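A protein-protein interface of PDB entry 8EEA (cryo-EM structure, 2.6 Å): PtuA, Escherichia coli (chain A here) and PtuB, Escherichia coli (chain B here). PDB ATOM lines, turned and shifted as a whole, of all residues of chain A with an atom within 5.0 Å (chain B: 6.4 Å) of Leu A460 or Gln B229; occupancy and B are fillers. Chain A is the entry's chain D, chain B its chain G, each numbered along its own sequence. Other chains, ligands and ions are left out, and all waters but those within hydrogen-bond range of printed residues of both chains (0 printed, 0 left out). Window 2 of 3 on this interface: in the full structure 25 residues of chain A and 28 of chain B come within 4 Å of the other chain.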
ATOM      1  N   ARG A 456      -5.397 -29.221  -1.406  1.00  0.00           N
ATOM      2  CA  ARG A 456      -6.181 -29.403  -0.188  1.00  0.00           C
ATOM      3  C   ARG A 456      -7.106 -28.216   0.056  1.00  0.00           C
ATOM      4  O   ARG A 456      -8.282 -28.392   0.397  1.00  0.00           O
ATOM      5  CB  ARG A 456      -5.244 -29.610   1.004  1.00  0.00           C
ATOM      6  CG  ARG A 456      -5.883 -29.413   2.371  1.00  0.00           C
ATOM      7  CD  ARG A 456      -4.857 -29.554   3.476  1.00  0.00           C
ATOM      8  NE  ARG A 456      -3.901 -28.454   3.469  1.00  0.00           N
ATOM      9  CZ  ARG A 456      -4.154 -27.235   3.924  1.00  0.00           C
ATOM     10  NH1 ARG A 456      -5.326 -26.922   4.448  1.00  0.00           N
ATOM     11  NH2 ARG A 456      -3.207 -26.304   3.847  1.00  0.00           N
ATOM     12  N   GLN A 457      -6.588 -26.997  -0.109  1.00  0.00           N
ATOM     13  CA  GLN A 457      -7.412 -25.814   0.115  1.00  0.00           C
ATOM     14  C   GLN A 457      -8.544 -25.735  -0.900  1.00  0.00           C
ATOM     15  O   GLN A 457      -9.661 -25.326  -0.563  1.00  0.00           O
ATOM     16  CB  GLN A 457      -6.548 -24.555   0.064  1.00  0.00           C
ATOM     17  CG  GLN A 457      -5.734 -24.330   1.325  1.00  0.00           C
ATOM     18  CD  GLN A 457      -4.725 -23.213   1.180  1.00  0.00           C
ATOM     19  OE1 GLN A 457      -4.991 -22.071   1.550  1.00  0.00           O
ATOM     20  NE2 GLN A 457      -3.556 -23.538   0.643  1.00  0.00           N
ATOM     21  N   ARG A 458      -8.277 -26.118  -2.150  1.00  0.00           N
ATOM     22  CA  ARG A 458      -9.344 -26.172  -3.144  1.00  0.00           C
ATOM     23  C   ARG A 458     -10.400 -27.201  -2.757  1.00  0.00           C
ATOM     24  O   ARG A 458     -11.602 -26.952  -2.903  1.00  0.00           O
ATOM     25  CB  ARG A 458      -8.765 -26.498  -4.520  1.00  0.00           C
ATOM     26  CG  ARG A 458      -8.223 -25.298  -5.273  1.00  0.00           C
ATOM     27  CD  ARG A 458      -8.136 -25.579  -6.765  1.00  0.00           C
ATOM     28  NE  ARG A 458      -7.653 -24.425  -7.513  1.00  0.00           N
ATOM     29  CZ  ARG A 458      -6.428 -24.296  -8.006  1.00  0.00           C
ATOM     30  NH1 ARG A 458      -5.511 -25.236  -7.848  1.00  0.00           N
ATOM     31  NH2 ARG A 458      -6.114 -23.191  -8.676  1.00  0.00           N
ATOM     32  N   LEU A 459      -9.967 -28.363  -2.268  1.00  0.00           N
ATOM     33  CA  LEU A 459     -10.913 -29.410  -1.897  1.00  0.00           C
ATOM     34  C   LEU A 459     -11.786 -28.986  -0.723  1.00  0.00           C
ATOM     35  O   LEU A 459     -12.985 -29.280  -0.698  1.00  0.00           O
ATOM     36  CB  LEU A 459     -10.162 -30.698  -1.563  1.00  0.00           C
ATOM     37  CG  LEU A 459     -11.031 -31.950  -1.429  1.00  0.00           C
ATOM     38  CD1 LEU A 459     -11.492 -32.433  -2.795  1.00  0.00           C
ATOM     39  CD2 LEU A 459     -10.279 -33.047  -0.698  1.00  0.00           C
ATOM     40  N   LEU A 460     -11.203 -28.299   0.262  1.00  0.00           N
ATOM     41  CA  LEU A 460     -11.962 -27.940   1.457  1.00  0.00           C
ATOM     42  C   LEU A 460     -13.147 -27.045   1.115  1.00  0.00           C
ATOM     43  O   LEU A 460     -14.241 -27.218   1.664  1.00  0.00           O
ATOM     44  CB  LEU A 460     -11.056 -27.250   2.476  1.00  0.00           C
ATOM     45  CG  LEU A 460     -10.176 -28.146   3.350  1.00  0.00           C
ATOM     46  CD1 LEU A 460      -9.301 -27.298   4.253  1.00  0.00           C
ATOM     47  CD2 LEU A 460     -11.017 -29.106   4.176  1.00  0.00           C
ATOM     48  N   LYS A 461     -12.952 -26.087   0.210  1.00  0.00           N
ATOM     49  CA  LYS A 461     -14.005 -25.138  -0.124  1.00  0.00           C
ATOM     50  C   LYS A 461     -15.081 -25.799  -0.975  1.00  0.00           C
ATOM     51  O   LYS A 461     -15.242 -25.468  -2.154  1.00  0.00           O
ATOM     52  CB  LYS A 461     -13.421 -23.927  -0.856  1.00  0.00           C
ATOM     53  CG  LYS A 461     -12.546 -23.045   0.016  1.00  0.00           C
ATOM     54  CD  LYS A 461     -11.972 -21.881  -0.772  1.00  0.00           C
ATOM     55  CE  LYS A 461     -11.043 -21.037   0.085  1.00  0.00           C
ATOM     56  NZ  LYS A 461      -9.770 -21.743   0.393  1.00  0.00           N
ATOM     57  N   GLY A 462     -15.817 -26.735  -0.385  1.00  0.00           N
ATOM     58  CA  GLY A 462     -16.876 -27.431  -1.090  1.00  0.00           C
ATOM     59  C   GLY A 462     -17.790 -28.191  -0.150  1.00  0.00           C
ATOM     60  O   GLY A 462     -17.407 -28.521   0.972  1.00  0.00           O
ATOM     61  N   PHE B 190      -5.210 -36.232   6.528  1.00  0.00           N
ATOM     62  CA  PHE B 190      -6.105 -35.773   5.470  1.00  0.00           C
ATOM     63  C   PHE B 190      -6.201 -36.806   4.355  1.00  0.00           C
ATOM     64  O   PHE B 190      -7.302 -37.194   3.940  1.00  0.00           O
ATOM     65  CB  PHE B 190      -5.616 -34.436   4.916  1.00  0.00           C
ATOM     66  CG  PHE B 190      -6.655 -33.693   4.127  1.00  0.00           C
ATOM     67  CD1 PHE B 190      -7.521 -32.813   4.749  1.00  0.00           C
ATOM     68  CD2 PHE B 190      -6.763 -33.878   2.759  1.00  0.00           C
ATOM     69  CE1 PHE B 190      -8.476 -32.132   4.021  1.00  0.00           C
ATOM     70  CE2 PHE B 190      -7.715 -33.199   2.028  1.00  0.00           C
ATOM     71  CZ  PHE B 190      -8.573 -32.326   2.659  1.00  0.00           C
ATOM     72  N   LEU B 200     -14.891 -36.549   8.791  1.00  0.00           N
ATOM     73  CA  LEU B 200     -13.888 -35.613   9.285  1.00  0.00           C
ATOM     74  C   LEU B 200     -14.371 -34.819  10.493  1.00  0.00           C
ATOM     75  O   LEU B 200     -13.952 -33.670  10.684  1.00  0.00           O
ATOM     76  CB  LEU B 200     -13.462 -34.671   8.157  1.00  0.00           C
ATOM     77  CG  LEU B 200     -12.153 -33.898   8.341  1.00  0.00           C
ATOM     78  CD1 LEU B 200     -10.975 -34.843   8.523  1.00  0.00           C
ATOM     79  CD2 LEU B 200     -11.924 -32.986   7.152  1.00  0.00           C
ATOM     80  N   ARG B 224      -6.338 -26.346  14.019  1.00  0.00           N
ATOM     81  CA  ARG B 224      -7.529 -25.554  13.729  1.00  0.00           C
ATOM     82  C   ARG B 224      -7.403 -24.839  12.388  1.00  0.00           C
ATOM     83  O   ARG B 224      -8.378 -24.737  11.636  1.00  0.00           O
ATOM     84  CB  ARG B 224      -7.779 -24.552  14.853  1.00  0.00           C
ATOM     85  CG  ARG B 224      -9.143 -23.893  14.791  1.00  0.00           C
ATOM     86  CD  ARG B 224      -9.336 -22.900  15.919  1.00  0.00           C
ATOM     87  NE  ARG B 224      -8.327 -21.849  15.900  1.00  0.00           N
ATOM     88  CZ  ARG B 224      -8.250 -20.869  16.790  1.00  0.00           C
ATOM     89  NH1 ARG B 224      -9.119 -20.763  17.780  1.00  0.00           N
ATOM     90  NH2 ARG B 224      -7.275 -19.971  16.680  1.00  0.00           N
ATOM     91  N   GLN B 225      -6.211 -24.330  12.075  1.00  0.00           N
ATOM     92  CA  GLN B 225      -5.995 -23.629  10.816  1.00  0.00           C
ATOM     93  C   GLN B 225      -5.905 -24.583   9.631  1.00  0.00           C
ATOM     94  O   GLN B 225      -6.240 -24.198   8.506  1.00  0.00           O
ATOM     95  CB  GLN B 225      -4.722 -22.789  10.912  1.00  0.00           C
ATOM     96  CG  GLN B 225      -4.541 -21.782   9.796  1.00  0.00           C
ATOM     97  CD  GLN B 225      -3.096 -21.363   9.626  1.00  0.00           C
ATOM     98  OE1 GLN B 225      -2.568 -20.583  10.418  1.00  0.00           O
ATOM     99  NE2 GLN B 225      -2.446 -21.884   8.592  1.00  0.00           N
ATOM    100  N   PHE B 226      -5.459 -25.821   9.860  1.00  0.00           N
ATOM    101  CA  PHE B 226      -5.308 -26.776   8.766  1.00  0.00           C
ATOM    102  C   PHE B 226      -6.660 -27.163   8.179  1.00  0.00           C
ATOM    103  O   PHE B 226      -6.837 -27.153   6.956  1.00  0.00           O
ATOM    104  CB  PHE B 226      -4.560 -28.010   9.268  1.00  0.00           C
ATOM    105  CG  PHE B 226      -4.092 -28.927   8.178  1.00  0.00           C
ATOM    106  CD1 PHE B 226      -4.884 -29.976   7.749  1.00  0.00           C
ATOM    107  CD2 PHE B 226      -2.851 -28.749   7.592  1.00  0.00           C
ATOM    108  CE1 PHE B 226      -4.452 -30.824   6.751  1.00  0.00           C
ATOM    109  CE2 PHE B 226      -2.414 -29.595   6.597  1.00  0.00           C
ATOM    110  CZ  PHE B 226      -3.215 -30.634   6.177  1.00  0.00           C
ATOM    111  N   PHE B 227      -7.618 -27.518   9.031  1.00  0.00           N
ATOM    112  CA  PHE B 227      -8.993 -27.788   8.617  1.00  0.00           C
ATOM    113  C   PHE B 227      -9.776 -26.498   8.835  1.00  0.00           C
ATOM    114  O   PHE B 227     -10.084 -26.130   9.970  1.00  0.00           O
ATOM    115  CB  PHE B 227      -9.583 -28.954   9.402  1.00  0.00           C
ATOM    116  CG  PHE B 227      -8.765 -30.210   9.326  1.00  0.00           C
ATOM    117  CD1 PHE B 227      -8.927 -31.097   8.279  1.00  0.00           C
ATOM    118  CD2 PHE B 227      -7.830 -30.503  10.304  1.00  0.00           C
ATOM    119  CE1 PHE B 227      -8.173 -32.251   8.207  1.00  0.00           C
ATOM    120  CE2 PHE B 227      -7.074 -31.656  10.237  1.00  0.00           C
ATOM    121  CZ  PHE B 227      -7.247 -32.531   9.187  1.00  0.00           C
ATOM    122  N   GLN B 228     -10.092 -25.811   7.740  1.00  0.00           N
ATOM    123  CA  GLN B 228     -10.573 -24.437   7.835  1.00  0.00           C
ATOM    124  C   GLN B 228     -11.951 -24.373   8.485  1.00  0.00           C
ATOM    125  O   GLN B 228     -12.123 -23.765   9.548  1.00  0.00           O
ATOM    126  CB  GLN B 228     -10.595 -23.809   6.442  1.00  0.00           C
ATOM    127  CG  GLN B 228      -9.208 -23.593   5.856  1.00  0.00           C
ATOM    128  CD  GLN B 228      -9.191 -23.628   4.341  1.00  0.00           C
ATOM    129  OE1 GLN B 228     -10.100 -24.161   3.708  1.00  0.00           O
ATOM    130  NE2 GLN B 228      -8.149 -23.056   3.751  1.00  0.00           N
ATOM    131  N   GLN B 229     -12.949 -24.999   7.862  1.00  0.00           N
ATOM    132  CA  GLN B 229     -14.323 -24.932   8.344  1.00  0.00           C
ATOM    133  C   GLN B 229     -14.738 -26.147   9.156  1.00  0.00           C
ATOM    134  O   GLN B 229     -15.595 -26.024  10.037  1.00  0.00           O
ATOM    135  CB  GLN B 229     -15.292 -24.770   7.168  1.00  0.00           C
ATOM    136  CG  GLN B 229     -14.823 -23.791   6.101  1.00  0.00           C
ATOM    137  CD  GLN B 229     -13.962 -24.443   5.037  1.00  0.00           C
ATOM    138  OE1 GLN B 229     -14.091 -25.634   4.759  1.00  0.00           O
ATOM    139  NE2 GLN B 229     -13.079 -23.660   4.429  1.00  0.00           N
ATOM    140  N   GLU B 230     -14.161 -27.318   8.880  1.00  0.00           N
ATOM    141  CA  GLU B 230     -14.496 -28.505   9.656  1.00  0.00           C
ATOM    142  C   GLU B 230     -14.089 -28.339  11.115  1.00  0.00           C
ATOM    143  O   GLU B 230     -14.836 -28.720  12.025  1.00  0.00           O
ATOM    144  CB  GLU B 230     -13.824 -29.735   9.045  1.00  0.00           C
ATOM    145  CG  GLU B 230     -14.107 -29.931   7.563  1.00  0.00           C
ATOM    146  CD  GLU B 230     -15.216 -30.930   7.307  1.00  0.00           C
ATOM    147  OE1 GLU B 230     -16.135 -31.030   8.149  1.00  0.00           O
ATOM    148  OE2 GLU B 230     -15.172 -31.616   6.265  1.00  0.00           O
ATOM    149  N   ALA B 231     -12.905 -27.769  11.356  1.00  0.00           N
ATOM    150  CA  ALA B 231     -12.466 -27.534  12.726  1.00  0.00           C
ATOM    151  C   ALA B 231     -13.395 -26.561  13.440  1.00  0.00           C
ATOM    152  O   ALA B 231     -13.731 -26.759  14.613  1.00  0.00           O
ATOM    153  CB  ALA B 231     -11.032 -27.006  12.732  1.00  0.00           C
ATOM    154  N   GLU B 232     -13.814 -25.497  12.751  1.00  0.00           N
ATOM    155  CA  GLU B 232     -14.734 -24.541  13.359  1.00  0.00           C
ATOM    156  C   GLU B 232     -16.070 -25.195  13.679  1.00  0.00           C
ATOM    157  O   GLU B 232     -16.659 -24.939  14.736  1.00  0.00           O
ATOM    158  CB  GLU B 232     -14.931 -23.342  12.432  1.00  0.00           C
ATOM    159  CG  GLU B 232     -13.666 -22.539  12.183  1.00  0.00           C
ATOM    160  CD  GLU B 232     -13.141 -21.868  13.438  1.00  0.00           C
ATOM    161  OE1 GLU B 232     -13.863 -21.858  14.456  1.00  0.00           O
ATOM    162  OE2 GLU B 232     -12.005 -21.350  13.407  1.00  0.00           O
ATOM    163  N   GLN B 233     -16.572 -26.037  12.774  1.00  0.00           N
ATOM    164  CA  GLN B 233     -17.819 -26.748  13.042  1.00  0.00           C
ATOM    165  C   GLN B 233     -17.681 -27.648  14.262  1.00  0.00           C
ATOM    166  O   GLN B 233     -18.566 -27.674  15.128  1.00  0.00           O
ATOM    167  CB  GLN B 233     -18.225 -27.566  11.816  1.00  0.00           C
ATOM    168  CG  GLN B 233     -19.554 -28.291  11.956  1.00  0.00           C
ATOM    169  CD  GLN B 233     -20.719 -27.343  12.154  1.00  0.00           C
ATOM    170  OE1 GLN B 233     -21.255 -27.220  13.255  1.00  0.00           O
ATOM    171  NE2 GLN B 233     -21.120 -26.667  11.084  1.00  0.00           N
ATOM    172  N   VAL B 234     -16.574 -28.384  14.355  1.00  0.00           N
ATOM    173  CA  VAL B 234     -16.361 -29.266  15.498  1.00  0.00           C
ATOM    174  C   VAL B 234     -16.311 -28.455  16.787  1.00  0.00           C
ATOM    175  O   VAL B 234     -16.918 -28.822  17.799  1.00  0.00           O
ATOM    176  CB  VAL B 234     -15.077 -30.096  15.306  1.00  0.00           C
ATOM    177  CG1 VAL B 234     -14.610 -30.675  16.632  1.00  0.00           C
ATOM    178  CG2 VAL B 234     -15.310 -31.200  14.288  1.00  0.00           C
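Arg A456 touches Phe B190. Gln A457 touches Gln B228. Leu A459 touches Phe B190. CD2 of Leu A460 touches CE1 of Phe B190, at 3.95 Å. Phe B226 touches Leu A460 (O to CD1, 3.7 Å). CD1 of Leu A460 touches OE1 of Gln B228, at 3.3 Å. Gln B228 touches Lys A461.
NH1 of Arg A456 lies within hydrogen-bond range of O of Phe B226 (2.9 Å). O of Leu A460 sits close to OE1 of Gln B229 (3.5 Å).
Of the printed residues of chain B, Gln A457 touches Gln B228 (3.7 Å). Of the printed residues of chain B, Lys A461 touches Gln B228 (3.95 Å). Printed residues of chain A within 4 Å of Phe B190: Arg A456 (3.98 Å), Leu A459 (3.7 Å) and Leu A460 (3.95 Å). Leu B200 touches none of the printed residues of chain A. Printed residues of chain A within 4 Å of Phe B226: Arg A456 (2.9 Å) and Leu A460 (3.7 Å). Of the printed residues of chain A, Gln B228 touches Gln A457, Leu A460 and Lys A461. Printed residues of chain A within 4 Å of Gln B229: Leu A460 (3.5 Å). Glu B230 touches none of the printed residues of chain A. The nearest residue of chain B that does not touch Leu A460 is Phe B227 (4.4 Å). The nearest residue of chain A that does not touch Gln B229 is Lys A461 (4.5 Å). The nearest printed residue of chain A that does not touch Phe B190 is Gln A457 (6.3 Å).
OE1 of Gln B228 is in hydrogen-bond range of NE2 of Gln B229 (3.1 Å).
Hydrophobic or aromatic side chains of chain B that line the printed part of chain A: Phe B190 and Phe B226. Among the printed residues, no Asp or Glu carboxylate lies within 4 Å of a Lys or Arg side-chain nitrogen of the other chain.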
